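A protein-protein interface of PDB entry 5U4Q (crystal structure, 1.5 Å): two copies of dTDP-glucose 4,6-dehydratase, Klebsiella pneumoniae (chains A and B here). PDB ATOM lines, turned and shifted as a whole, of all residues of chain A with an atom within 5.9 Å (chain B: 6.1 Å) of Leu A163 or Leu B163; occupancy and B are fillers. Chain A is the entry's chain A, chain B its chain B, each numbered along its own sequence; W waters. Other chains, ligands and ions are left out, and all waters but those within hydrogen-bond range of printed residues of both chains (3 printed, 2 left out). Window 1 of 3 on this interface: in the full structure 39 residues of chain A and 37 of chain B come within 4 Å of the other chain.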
ATOM      1  N   TYR A 126      -9.873  32.793 -23.576  1.00  0.00           N
ATOM      2  CA  TYR A 126     -11.141  33.100 -24.249  1.00  0.00           C
ATOM      3  C   TYR A 126     -11.896  34.146 -23.478  1.00  0.00           C
ATOM      4  O   TYR A 126     -11.740  34.274 -22.263  1.00  0.00           O
ATOM      5  CB  TYR A 126     -11.999  31.818 -24.475  1.00  0.00           C
ATOM      6  CG  TYR A 126     -12.417  31.161 -23.186  1.00  0.00           C
ATOM      7  CD1 TYR A 126     -11.544  30.319 -22.507  1.00  0.00           C
ATOM      8  CD2 TYR A 126     -13.665  31.422 -22.599  1.00  0.00           C
ATOM      9  CE1 TYR A 126     -11.886  29.751 -21.286  1.00  0.00           C
ATOM     10  CE2 TYR A 126     -14.023  30.838 -21.390  1.00  0.00           C
ATOM     11  CZ  TYR A 126     -13.125  30.031 -20.719  1.00  0.00           C
ATOM     12  OH  TYR A 126     -13.461  29.496 -19.496  1.00  0.00           O
ATOM     13  N   VAL A 147     -22.600  31.887 -10.334  1.00  0.00           N
ATOM     14  CA  VAL A 147     -22.937  32.506 -11.605  1.00  0.00           C
ATOM     15  C   VAL A 147     -23.914  31.556 -12.320  1.00  0.00           C
ATOM     16  O   VAL A 147     -23.680  31.112 -13.439  1.00  0.00           O
ATOM     17  CB  VAL A 147     -21.649  32.800 -12.421  1.00  0.00           C
ATOM     18  CG1 VAL A 147     -20.898  33.972 -11.800  1.00  0.00           C
ATOM     19  CG2 VAL A 147     -20.728  31.598 -12.466  1.00  0.00           C
ATOM     20  N   ASP A 148     -24.991  31.258 -11.605  1.00  0.00           N
ATOM     21  CA  ASP A 148     -26.067  30.344 -12.012  1.00  0.00           C
ATOM     22  C   ASP A 148     -27.345  31.008 -12.490  1.00  0.00           C
ATOM     23  O   ASP A 148     -28.276  30.300 -12.915  1.00  0.00           O
ATOM     24  CB  ASP A 148     -26.502  29.554 -10.760  1.00  0.00           C
ATOM     25  CG  ASP A 148     -25.452  28.643 -10.266  1.00  0.00           C
ATOM     26  OD1 ASP A 148     -25.046  27.772 -11.058  1.00  0.00           O
ATOM     27  OD2 ASP A 148     -25.064  28.763  -9.082  1.00  0.00           O
ATOM     28  N   HIS A 149     -27.411  32.324 -12.401  1.00  0.00           N
ATOM     29  CA  HIS A 149     -28.670  33.037 -12.650  1.00  0.00           C
ATOM     30  C   HIS A 149     -28.522  34.145 -13.651  1.00  0.00           C
ATOM     31  O   HIS A 149     -28.733  35.311 -13.346  1.00  0.00           O
ATOM     32  CB  HIS A 149     -29.201  33.594 -11.316  1.00  0.00           C
ATOM     33  CG  HIS A 149     -29.526  32.543 -10.321  1.00  0.00           C
ATOM     34  ND1 HIS A 149     -28.646  32.165  -9.331  1.00  0.00           N
ATOM     35  CD2 HIS A 149     -30.640  31.791 -10.148  1.00  0.00           C
ATOM     36  CE1 HIS A 149     -29.196  31.207  -8.605  1.00  0.00           C
ATOM     37  NE2 HIS A 149     -30.406  30.960  -9.082  1.00  0.00           N
ATOM     38  N   PRO A 150     -28.145  33.788 -14.893  1.00  0.00           N
ATOM     39  CA  PRO A 150     -27.991  34.814 -15.898  1.00  0.00           C
ATOM     40  C   PRO A 150     -29.310  35.484 -16.270  1.00  0.00           C
ATOM     41  O   PRO A 150     -30.368  34.841 -16.235  1.00  0.00           O
ATOM     42  CB  PRO A 150     -27.414  34.032 -17.108  1.00  0.00           C
ATOM     43  CG  PRO A 150     -27.923  32.658 -16.912  1.00  0.00           C
ATOM     44  CD  PRO A 150     -27.897  32.441 -15.428  1.00  0.00           C
ATOM     45  N   ALA A 156     -25.770  33.752 -20.485  1.00  0.00           N
ATOM     46  CA  ALA A 156     -25.885  32.300 -20.415  1.00  0.00           C
ATOM     47  C   ALA A 156     -24.884  31.631 -21.356  1.00  0.00           C
ATOM     48  O   ALA A 156     -24.313  30.609 -20.996  1.00  0.00           O
ATOM     49  CB  ALA A 156     -27.279  31.848 -20.741  1.00  0.00           C
ATOM     50  N   LYS A 158     -21.963  32.810 -22.345  1.00  0.00           N
ATOM     51  CA  LYS A 158     -20.620  32.974 -21.804  1.00  0.00           C
ATOM     52  C   LYS A 158     -20.346  32.002 -20.655  1.00  0.00           C
ATOM     53  O   LYS A 158     -19.245  31.415 -20.561  1.00  0.00           O
ATOM     54  CB  LYS A 158     -20.331  34.436 -21.444  1.00  0.00           C
ATOM     55  CG  LYS A 158     -20.271  35.381 -22.654  1.00  0.00           C
ATOM     56  CD  LYS A 158     -19.229  34.948 -23.698  1.00  0.00           C
ATOM     57  CE  LYS A 158     -18.811  36.110 -24.603  1.00  0.00           C
ATOM     58  NZ  LYS A 158     -17.701  35.726 -25.560  1.00  0.00           N
ATOM     59  N   LYS A 159     -21.324  31.818 -19.762  1.00  0.00           N
ATOM     60  CA  LYS A 159     -21.167  30.825 -18.711  1.00  0.00           C
ATOM     61  C   LYS A 159     -21.089  29.434 -19.335  1.00  0.00           C
ATOM     62  O   LYS A 159     -20.294  28.606 -18.894  1.00  0.00           O
ATOM     63  CB  LYS A 159     -22.270  30.918 -17.651  1.00  0.00           C
ATOM     64  CG  LYS A 159     -22.207  29.851 -16.592  1.00  0.00           C
ATOM     65  CD  LYS A 159     -20.893  29.717 -15.787  1.00  0.00           C
ATOM     66  CE  LYS A 159     -21.085  28.558 -14.786  1.00  0.00           C
ATOM     67  NZ  LYS A 159     -19.893  28.138 -14.002  1.00  0.00           N
ATOM     68  N   ALA A 160     -21.886  29.189 -20.376  1.00  0.00           N
ATOM     69  CA  ALA A 160     -21.774  27.913 -21.063  1.00  0.00           C
ATOM     70  C   ALA A 160     -20.360  27.701 -21.597  1.00  0.00           C
ATOM     71  O   ALA A 160     -19.864  26.568 -21.574  1.00  0.00           O
ATOM     72  CB  ALA A 160     -22.795  27.772 -22.188  1.00  0.00           C
ATOM     73  N   ASN A 161     -19.728  28.754 -22.114  1.00  0.00           N
ATOM     74  CA  ASN A 161     -18.326  28.636 -22.614  1.00  0.00           C
ATOM     75  C   ASN A 161     -17.420  28.203 -21.461  1.00  0.00           C
ATOM     76  O   ASN A 161     -16.571  27.315 -21.639  1.00  0.00           O
ATOM     77  CB  ASN A 161     -17.810  29.961 -23.155  1.00  0.00           C
ATOM     78  CG  ASN A 161     -18.437  30.399 -24.496  1.00  0.00           C
ATOM     79  OD1 ASN A 161     -18.025  31.436 -25.015  1.00  0.00           O
ATOM     80  ND2 ASN A 161     -19.292  29.596 -25.092  1.00  0.00           N
ATOM     81  N   GLU A 162     -17.596  28.800 -20.284  1.00  0.00           N
ATOM     82  CA  GLU A 162     -16.764  28.419 -19.122  1.00  0.00           C
ATOM     83  C   GLU A 162     -16.974  26.938 -18.778  1.00  0.00           C
ATOM     84  O   GLU A 162     -16.011  26.227 -18.472  1.00  0.00           O
ATOM     85  CB  GLU A 162     -17.043  29.324 -17.920  1.00  0.00           C
ATOM     86  CG  GLU A 162     -16.722  30.803 -18.143  1.00  0.00           C
ATOM     87  CD  GLU A 162     -16.967  31.668 -16.930  1.00  0.00           C
ATOM     88  OE1 GLU A 162     -17.206  31.122 -15.815  1.00  0.00           O
ATOM     89  OE2 GLU A 162     -16.904  32.920 -17.056  1.00  0.00           O
ATOM     90  N   LEU A 163     -18.234  26.484 -18.848  1.00  0.00           N
ATOM     91  CA  LEU A 163     -18.549  25.082 -18.526  1.00  0.00           C
ATOM     92  C   LEU A 163     -17.914  24.137 -19.517  1.00  0.00           C
ATOM     93  O   LEU A 163     -17.360  23.099 -19.140  1.00  0.00           O
ATOM     94  CB  LEU A 163     -20.055  24.855 -18.482  1.00  0.00           C
ATOM     95  CG  LEU A 163     -20.806  25.507 -17.317  1.00  0.00           C
ATOM     96  CD1 LEU A 163     -22.267  25.632 -17.687  1.00  0.00           C
ATOM     97  CD2 LEU A 163     -20.602  24.734 -16.018  1.00  0.00           C
ATOM     98  N   MET A 164     -17.992  24.504 -20.796  1.00  0.00           N
ATOM     99  CA  MET A 164     -17.416  23.700 -21.862  1.00  0.00           C
ATOM    100  C   MET A 164     -15.903  23.673 -21.735  1.00  0.00           C
ATOM    101  O   MET A 164     -15.280  22.623 -21.899  1.00  0.00           O
ATOM    102  CB  MET A 164     -17.909  24.224 -23.221  1.00  0.00           C
ATOM    103  CG  MET A 164     -19.432  24.071 -23.346  1.00  0.00           C
ATOM    104  SD  MET A 164     -20.212  25.256 -24.727  1.00  0.00           S
ATOM    105  CE  MET A 164     -19.466  24.420 -26.332  1.00  0.00           C
ATOM    106  N   ALA A 165     -15.293  24.822 -21.432  1.00  0.00           N
ATOM    107  CA  ALA A 165     -13.846  24.896 -21.216  1.00  0.00           C
ATOM    108  C   ALA A 165     -13.443  23.951 -20.071  1.00  0.00           C
ATOM    109  O   ALA A 165     -12.461  23.194 -20.198  1.00  0.00           O
ATOM    110  CB  ALA A 165     -13.391  26.323 -20.904  1.00  0.00           C
ATOM    111  N   HIS A 166     -14.227  23.954 -19.006  1.00  0.00           N
ATOM    112  CA  HIS A 166     -13.903  23.088 -17.856  1.00  0.00           C
ATOM    113  C   HIS A 166     -13.862  21.624 -18.294  1.00  0.00           C
ATOM    114  O   HIS A 166     -12.912  20.892 -17.972  1.00  0.00           O
ATOM    115  CB  HIS A 166     -14.897  23.215 -16.728  1.00  0.00           C
ATOM    116  CG  HIS A 166     -14.496  22.401 -15.555  1.00  0.00           C
ATOM    117  ND1 HIS A 166     -14.946  21.110 -15.344  1.00  0.00           N
ATOM    118  CD2 HIS A 166     -13.561  22.640 -14.605  1.00  0.00           C
ATOM    119  CE1 HIS A 166     -14.314  20.604 -14.298  1.00  0.00           C
ATOM    120  NE2 HIS A 166     -13.484  21.515 -13.819  1.00  0.00           N
ATOM    121  N   THR A 167     -14.890  21.191 -19.034  1.00  0.00           N
ATOM    122  CA  THR A 167     -14.927  19.795 -19.494  1.00  0.00           C
ATOM    123  C   THR A 167     -13.753  19.418 -20.415  1.00  0.00           C
ATOM    124  O   THR A 167     -13.223  18.329 -20.314  1.00  0.00           O
ATOM    125  CB  THR A 167     -16.258  19.407 -20.218  1.00  0.00           C
ATOM    126  OG1 THR A 167     -16.310  20.005 -21.508  1.00  0.00           O
ATOM    127  CG2 THR A 167     -17.457  19.793 -19.446  1.00  0.00           C
ATOM    128  N   TYR A 168     -13.339  20.315 -21.299  1.00  0.00           N
ATOM    129  CA  TYR A 168     -12.221  20.039 -22.192  1.00  0.00           C
ATOM    130  C   TYR A 168     -10.883  20.040 -21.443  1.00  0.00           C
ATOM    131  O   TYR A 168      -9.989  19.225 -21.755  1.00  0.00           O
ATOM    132  CB  TYR A 168     -12.262  20.977 -23.413  1.00  0.00           C
ATOM    133  CG  TYR A 168     -13.105  20.388 -24.514  1.00  0.00           C
ATOM    134  CD1 TYR A 168     -14.448  20.107 -24.320  1.00  0.00           C
ATOM    135  CD2 TYR A 168     -12.544  20.056 -25.736  1.00  0.00           C
ATOM    136  CE1 TYR A 168     -15.208  19.494 -25.311  1.00  0.00           C
ATOM    137  CE2 TYR A 168     -13.305  19.472 -26.741  1.00  0.00           C
ATOM    138  CZ  TYR A 168     -14.629  19.176 -26.512  1.00  0.00           C
ATOM    139  OH  TYR A 168     -15.407  18.564 -27.476  1.00  0.00           O
ATOM    140  N   TYR A 258      -7.737  24.654 -15.589  1.00  0.00           N
ATOM    141  CA  TYR A 258      -8.850  25.539 -15.919  1.00  0.00           C
ATOM    142  C   TYR A 258      -8.874  26.701 -14.956  1.00  0.00           C
ATOM    143  O   TYR A 258      -8.830  26.512 -13.732  1.00  0.00           O
ATOM    144  CB  TYR A 258     -10.154  24.761 -15.775  1.00  0.00           C
ATOM    145  CG  TYR A 258     -11.443  25.558 -15.545  1.00  0.00           C
ATOM    146  CD1 TYR A 258     -12.256  25.935 -16.628  1.00  0.00           C
ATOM    147  CD2 TYR A 258     -11.896  25.866 -14.264  1.00  0.00           C
ATOM    148  CE1 TYR A 258     -13.434  26.637 -16.423  1.00  0.00           C
ATOM    149  CE2 TYR A 258     -13.087  26.562 -14.047  1.00  0.00           C
ATOM    150  CZ  TYR A 258     -13.868  26.923 -15.140  1.00  0.00           C
ATOM    151  OH  TYR A 258     -15.048  27.613 -14.917  1.00  0.00           O
ATOM    152  N   TYR B 126     -38.243  20.175 -18.551  1.00  0.00           N
ATOM    153  CA  TYR B 126     -37.196  19.638 -19.423  1.00  0.00           C
ATOM    154  C   TYR B 126     -36.252  18.750 -18.654  1.00  0.00           C
ATOM    155  O   TYR B 126     -36.084  18.907 -17.432  1.00  0.00           O
ATOM    156  CB  TYR B 126     -36.409  20.792 -20.086  1.00  0.00           C
ATOM    157  CG  TYR B 126     -35.720  21.691 -19.081  1.00  0.00           C
ATOM    158  CD1 TYR B 126     -36.404  22.710 -18.448  1.00  0.00           C
ATOM    159  CD2 TYR B 126     -34.365  21.521 -18.771  1.00  0.00           C
ATOM    160  CE1 TYR B 126     -35.786  23.514 -17.502  1.00  0.00           C
ATOM    161  CE2 TYR B 126     -33.730  22.325 -17.838  1.00  0.00           C
ATOM    162  CZ  TYR B 126     -34.449  23.325 -17.204  1.00  0.00           C
ATOM    163  OH  TYR B 126     -33.858  24.131 -16.234  1.00  0.00           O
ATOM    164  N   VAL B 147     -22.836  23.641  -9.300  1.00  0.00           N
ATOM    165  CA  VAL B 147     -22.668  22.659 -10.378  1.00  0.00           C
ATOM    166  C   VAL B 147     -21.888  23.326 -11.533  1.00  0.00           C
ATOM    167  O   VAL B 147     -22.382  23.483 -12.637  1.00  0.00           O
ATOM    168  CB  VAL B 147     -24.043  22.099 -10.842  1.00  0.00           C
ATOM    169  CG1 VAL B 147     -24.556  21.112  -9.797  1.00  0.00           C
ATOM    170  CG2 VAL B 147     -25.026  23.233 -11.034  1.00  0.00           C
ATOM    171  N   ASP B 148     -20.659  23.705 -11.224  1.00  0.00           N
ATOM    172  CA  ASP B 148     -19.772  24.431 -12.122  1.00  0.00           C
ATOM    173  C   ASP B 148     -18.655  23.612 -12.733  1.00  0.00           C
ATOM    174  O   ASP B 148     -17.874  24.141 -13.531  1.00  0.00           O
ATOM    175  CB  ASP B 148     -19.104  25.569 -11.297  1.00  0.00           C
ATOM    176  CG  ASP B 148     -20.093  26.533 -10.745  1.00  0.00           C
ATOM    177  OD1 ASP B 148     -20.822  27.124 -11.571  1.00  0.00           O
ATOM    178  OD2 ASP B 148     -20.135  26.736  -9.484  1.00  0.00           O
ATOM    179  N   HIS B 149     -18.558  22.328 -12.393  1.00  0.00           N
ATOM    180  CA  HIS B 149     -17.393  21.530 -12.775  1.00  0.00           C
ATOM    181  C   HIS B 149     -17.758  20.245 -13.466  1.00  0.00           C
ATOM    182  O   HIS B 149     -17.434  19.175 -13.000  1.00  0.00           O
ATOM    183  CB  HIS B 149     -16.545  21.260 -11.531  1.00  0.00           C
ATOM    184  CG  HIS B 149     -16.050  22.511 -10.901  1.00  0.00           C
ATOM    185  ND1 HIS B 149     -16.729  23.138  -9.877  1.00  0.00           N
ATOM    186  CD2 HIS B 149     -14.990  23.297 -11.205  1.00  0.00           C
ATOM    187  CE1 HIS B 149     -16.087  24.257  -9.563  1.00  0.00           C
ATOM    188  NE2 HIS B 149     -15.030  24.373 -10.351  1.00  0.00           N
ATOM    189  N   PRO B 150     -18.469  20.351 -14.608  1.00  0.00           N
ATOM    190  CA  PRO B 150     -18.818  19.150 -15.347  1.00  0.00           C
ATOM    191  C   PRO B 150     -17.607  18.430 -15.895  1.00  0.00           C
ATOM    192  O   PRO B 150     -16.607  19.061 -16.207  1.00  0.00           O
ATOM    193  CB  PRO B 150     -19.694  19.697 -16.503  1.00  0.00           C
ATOM    194  CG  PRO B 150     -19.160  21.071 -16.711  1.00  0.00           C
ATOM    195  CD  PRO B 150     -18.894  21.570 -15.322  1.00  0.00           C
ATOM    196  N   ALA B 156     -22.098  19.388 -19.457  1.00  0.00           N
ATOM    197  CA  ALA B 156     -22.013  20.812 -19.700  1.00  0.00           C
ATOM    198  C   ALA B 156     -23.251  21.287 -20.472  1.00  0.00           C
ATOM    199  O   ALA B 156     -23.786  22.353 -20.171  1.00  0.00           O
ATOM    200  CB  ALA B 156     -20.742  21.150 -20.462  1.00  0.00           C
ATOM    201  N   LYS B 158     -26.263  19.948 -20.412  1.00  0.00           N
ATOM    202  CA  LYS B 158     -27.423  19.932 -19.541  1.00  0.00           C
ATOM    203  C   LYS B 158     -27.431  21.103 -18.587  1.00  0.00           C
ATOM    204  O   LYS B 158     -28.474  21.715 -18.366  1.00  0.00           O
ATOM    205  CB  LYS B 158     -27.594  18.589 -18.831  1.00  0.00           C
ATOM    206  CG  LYS B 158     -27.917  17.423 -19.755  1.00  0.00           C
ATOM    207  CD  LYS B 158     -29.193  17.651 -20.526  1.00  0.00           C
ATOM    208  CE  LYS B 158     -29.777  16.379 -21.085  1.00  0.00           C
ATOM    209  NZ  LYS B 158     -31.092  16.664 -21.755  1.00  0.00           N
ATOM    210  N   LYS B 159     -26.265  21.470 -18.040  1.00  0.00           N
ATOM    211  CA  LYS B 159     -26.227  22.649 -17.200  1.00  0.00           C
ATOM    212  C   LYS B 159     -26.543  23.891 -18.044  1.00  0.00           C
ATOM    213  O   LYS B 159     -27.205  24.814 -17.570  1.00  0.00           O
ATOM    214  CB  LYS B 159     -24.872  22.803 -16.471  1.00  0.00           C
ATOM    215  CG  LYS B 159     -24.772  24.055 -15.596  1.00  0.00           C
ATOM    216  CD  LYS B 159     -25.845  24.105 -14.520  1.00  0.00           C
ATOM    217  CE  LYS B 159     -26.068  25.482 -13.946  1.00  0.00           C
ATOM    218  NZ  LYS B 159     -27.342  25.483 -13.155  1.00  0.00           N
ATOM    219  N   ALA B 160     -26.070  23.928 -19.290  1.00  0.00           N
ATOM    220  CA  ALA B 160     -26.368  25.039 -20.169  1.00  0.00           C
ATOM    221  C   ALA B 160     -27.878  25.163 -20.403  1.00  0.00           C
ATOM    222  O   ALA B 160     -28.380  26.252 -20.486  1.00  0.00           O
ATOM    223  CB  ALA B 160     -25.620  24.919 -21.486  1.00  0.00           C
ATOM    224  N   ASN B 161     -28.581  24.029 -20.476  1.00  0.00           N
ATOM    225  CA  ASN B 161     -30.045  24.069 -20.590  1.00  0.00           C
ATOM    226  C   ASN B 161     -30.644  24.786 -19.350  1.00  0.00           C
ATOM    227  O   ASN B 161     -31.531  25.630 -19.466  1.00  0.00           O
ATOM    228  CB  ASN B 161     -30.624  22.672 -20.655  1.00  0.00           C
ATOM    229  CG  ASN B 161     -30.387  21.944 -21.975  1.00  0.00           C
ATOM    230  OD1 ASN B 161     -30.936  20.866 -22.146  1.00  0.00           O
ATOM    231  ND2 ASN B 161     -29.598  22.507 -22.890  1.00  0.00           N
ATOM    232  N   GLU B 162     -30.141  24.444 -18.149  1.00  0.00           N
ATOM    233  CA  GLU B 162     -30.638  25.122 -16.938  1.00  0.00           C
ATOM    234  C   GLU B 162     -30.362  26.620 -16.980  1.00  0.00           C
ATOM    235  O   GLU B 162     -31.213  27.439 -16.643  1.00  0.00           O
ATOM    236  CB  GLU B 162     -30.041  24.491 -15.675  1.00  0.00           C
ATOM    237  CG  GLU B 162     -30.331  22.995 -15.511  1.00  0.00           C
ATOM    238  CD  GLU B 162     -29.779  22.382 -14.221  1.00  0.00           C
ATOM    239  OE1 GLU B 162     -29.229  23.136 -13.380  1.00  0.00           O
ATOM    240  OE2 GLU B 162     -29.859  21.146 -14.066  1.00  0.00           O
ATOM    241  N   LEU B 163     -29.179  27.014 -17.443  1.00  0.00           N
ATOM    242  CA  LEU B 163     -28.860  28.432 -17.522  1.00  0.00           C
ATOM    243  C   LEU B 163     -29.760  29.179 -18.511  1.00  0.00           C
ATOM    244  O   LEU B 163     -30.210  30.312 -18.239  1.00  0.00           O
ATOM    245  CB  LEU B 163     -27.409  28.643 -17.972  1.00  0.00           C
ATOM    246  CG  LEU B 163     -26.279  28.228 -17.037  1.00  0.00           C
ATOM    247  CD1 LEU B 163     -24.980  28.192 -17.847  1.00  0.00           C
ATOM    248  CD2 LEU B 163     -26.169  29.147 -15.816  1.00  0.00           C
ATOM    249  N   MET B 164     -30.003  28.543 -19.659  1.00  0.00           N
ATOM    250  CA  MET B 164     -30.837  29.114 -20.713  1.00  0.00           C
ATOM    251  C   MET B 164     -32.273  29.209 -20.234  1.00  0.00           C
ATOM    252  O   MET B 164     -32.935  30.205 -20.484  1.00  0.00           O
ATOM    253  CB  MET B 164     -30.662  28.263 -21.972  1.00  0.00           C
ATOM    254  CG  MET B 164     -29.230  28.412 -22.513  1.00  0.00           C
ATOM    255  SD  MET B 164     -28.725  26.952 -23.737  1.00  0.00           S
ATOM    256  CE  MET B 164     -29.790  27.505 -25.279  1.00  0.00           C
ATOM    257  N   ALA B 165     -32.728  28.183 -19.521  1.00  0.00           N
ATOM    258  CA  ALA B 165     -34.079  28.160 -18.915  1.00  0.00           C
ATOM    259  C   ALA B 165     -34.200  29.335 -17.950  1.00  0.00           C
ATOM    260  O   ALA B 165     -35.208  30.066 -17.970  1.00  0.00           O
ATOM    261  CB  ALA B 165     -34.331  26.863 -18.177  1.00  0.00           C
ATOM    262  N   HIS B 166     -33.183  29.520 -17.089  1.00  0.00           N
ATOM    263  CA  HIS B 166     -33.229  30.656 -16.152  1.00  0.00           C
ATOM    264  C   HIS B 166     -33.399  31.977 -16.880  1.00  0.00           C
ATOM    265  O   HIS B 166     -34.232  32.834 -16.505  1.00  0.00           O
ATOM    266  CB  HIS B 166     -31.988  30.743 -15.242  1.00  0.00           C
ATOM    267  CG  HIS B 166     -32.108  31.835 -14.234  1.00  0.00           C
ATOM    268  ND1 HIS B 166     -31.662  33.112 -14.466  1.00  0.00           N
ATOM    269  CD2 HIS B 166     -32.765  31.875 -13.048  1.00  0.00           C
ATOM    270  CE1 HIS B 166     -32.007  33.888 -13.449  1.00  0.00           C
ATOM    271  NE2 HIS B 166     -32.666  33.158 -12.571  1.00  0.00           N
ATOM    272  N   THR B 167     -32.574  32.209 -17.906  1.00  0.00           N
ATOM    273  CA  THR B 167     -32.616  33.420 -18.707  1.00  0.00           C
ATOM    274  C   THR B 167     -34.020  33.681 -19.282  1.00  0.00           C
ATOM    275  O   THR B 167     -34.527  34.791 -19.240  1.00  0.00           O
ATOM    276  CB  THR B 167     -31.607  33.329 -19.883  1.00  0.00           C
ATOM    277  OG1 THR B 167     -30.282  33.164 -19.348  1.00  0.00           O
ATOM    278  CG2 THR B 167     -31.653  34.545 -20.751  1.00  0.00           C
ATOM    279  N   TYR B 168     -34.626  32.635 -19.816  1.00  0.00           N
ATOM    280  CA  TYR B 168     -35.939  32.770 -20.453  1.00  0.00           C
ATOM    281  C   TYR B 168     -37.038  32.949 -19.406  1.00  0.00           C
ATOM    282  O   TYR B 168     -37.966  33.722 -19.641  1.00  0.00           O
ATOM    283  CB  TYR B 168     -36.187  31.618 -21.439  1.00  0.00           C
ATOM    284  CG  TYR B 168     -35.642  31.951 -22.809  1.00  0.00           C
ATOM    285  CD1 TYR B 168     -34.273  32.166 -23.026  1.00  0.00           C
ATOM    286  CD2 TYR B 168     -36.493  32.100 -23.901  1.00  0.00           C
ATOM    287  CE1 TYR B 168     -33.792  32.501 -24.292  1.00  0.00           C
ATOM    288  CE2 TYR B 168     -36.025  32.422 -25.152  1.00  0.00           C
ATOM    289  CZ  TYR B 168     -34.682  32.620 -25.359  1.00  0.00           C
ATOM    290  OH  TYR B 168     -34.245  32.976 -26.612  1.00  0.00           O
ATOM    291  N   TYR B 258     -38.554  29.849 -12.151  1.00  0.00           N
ATOM    292  CA  TYR B 258     -37.557  28.852 -12.508  1.00  0.00           C
ATOM    293  C   TYR B 258     -37.289  27.901 -11.364  1.00  0.00           C
ATOM    294  O   TYR B 258     -37.056  28.342 -10.230  1.00  0.00           O
ATOM    295  CB  TYR B 258     -36.264  29.609 -12.871  1.00  0.00           C
ATOM    296  CG  TYR B 258     -34.957  28.831 -12.810  1.00  0.00           C
ATOM    297  CD1 TYR B 258     -34.226  28.746 -11.617  1.00  0.00           C
ATOM    298  CD2 TYR B 258     -34.408  28.243 -13.948  1.00  0.00           C
ATOM    299  CE1 TYR B 258     -33.020  28.076 -11.564  1.00  0.00           C
ATOM    300  CE2 TYR B 258     -33.199  27.561 -13.901  1.00  0.00           C
ATOM    301  CZ  TYR B 258     -32.500  27.488 -12.716  1.00  0.00           C
ATOM    302  OH  TYR B 258     -31.292  26.824 -12.649  1.00  0.00           O
HETATM  303  O   HOH W   1     -28.867  27.800 -13.858  1.00  0.00           O
HETATM  304  O   HOH W   2     -22.160  29.063 -10.377  1.00  0.00           O
HETATM  305  O   HOH W   3     -17.700  26.456 -15.177  1.00  0.00           O
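The backbone carbonyl oxygen of Leu B163 is in hydrogen-bond range of the side-chain hydroxyl of Thr B167, 3.1 Å away.
The backbone carbonyl oxygen of Met A164 is in hydrogen-bond range of the side-chain hydroxyl of Thr A167, 2.8 Å away.
NZ of Lys B159 is in salt-bridge range of OE1 of Glu B162.
ND1 of His A166 lies within hydrogen-bond range of O of Pro B150 (2.8 Å).
The backbone carbonyl oxygen (O) of Pro A150 sits at hydrogen-bond distance from a ring nitrogen (ND1) of His B166.
OD1 of Asp B148 lies within salt-bridge range of NZ of Lys A159.
The side-chain carboxylate (OD1) of Asp A148 is in salt-bridge range of the side-chain amino group (NZ) of Lys B159 (3.9 Å).
Of the 18 printed residues of chain A, 9 touch a printed residue of chain B.
Printed residues of chain A that touch a printed residue of chain B: Val A147, Asp A148, His A149, Pro A150, Ala A156, Lys A159, Leu A163, His A166 and Thr A167.
Hydrophobic or aromatic side chains of chain A that line the printed part of chain B: His A149, Pro A150, Ala A156, Leu A163 and His A166.
Along chain A the printed residues that touch a printed residue of chain B span positions 147 to 167.
Of the 18 printed residues of chain B, 8 touch a printed residue of chain A.
Hydrophobic or aromatic side chains of chain B within 4 Å of the printed part of chain A: His B149, Pro B150, Ala B156, Leu B163 and His B166.
Among the printed residues, 18 pairs touch across the chains.
Among the printed residues, Asp or Glu carboxylates within 4 Å of a Lys or Arg side-chain nitrogen of the other chain: Asp A148 with Lys B159 and Lys A159 with Asp B148.
Water W2 lies within hydrogen-bond range of OD1 of Asp B148, N of Val A147 and OD2 of Asp A148.
Water W1 lies within hydrogen-bond range of O of Asp A148 (2.7 Å), NZ of Lys B159 (2.9 Å) and OH of Tyr B258 (2.9 Å).
Water W3 lies within hydrogen-bond range of O of Asp B148 (2.8 Å), OH of Tyr A258 (2.9 Å) and NZ of Lys A159 (3.0 Å).
Of chain B, only Asp B148, Pro B150, Lys B159 and Leu B163 come within 4 Å of Leu A163.
Leu B163 touches just these residues of chain A: Val A147 (3.96 Å), Asp A148 (3.8 Å), Pro A150 (3.5 Å), Lys A159 (3.5 Å) and Leu A163 (3.7 Å).
Of the printed residues of chain B, Lys A159 touches Asp B148 and Leu B163.
Of the printed residues of chain A, His B149 touches His A166.
Tyr B258 touches none of the printed residues of chain A.
Ala A160 touches none of the printed residues of chain B.
The nearest residue of chain B that does not touch Leu A163 is Val B147 (4.02 Å).
Among the printed residues, pairs that only touch across the chains: His A149 with His B166, Thr A167 with Pro B150, Pro A150 with Thr B167, Lys A159 with Leu B163, His A166 with His B149, Pro A150 with Leu B163, Ala A156 with Thr B167, Leu A163 with Lys B159, Leu A163 with Pro B150, Thr A167 with Ala B156, Leu A163 with Leu B163, Leu A163 with Asp B148, Asp A148 with Leu B163 and Val A147 with Leu B163.
Pro A150 touches His B166, and with the chains exchanged His A166 touches Pro B150.
Ala A156 touches Thr B167, and with the chains exchanged Thr A167 touches Ala B156.
Leu A163 touches its own counterpart, Leu B163.
Positions printed for both chains: 126, 147, 148, 149, 150, 156, 158, 159, 160, 161, 162, 163, 164, 165, 166, 167, 168 and 258.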
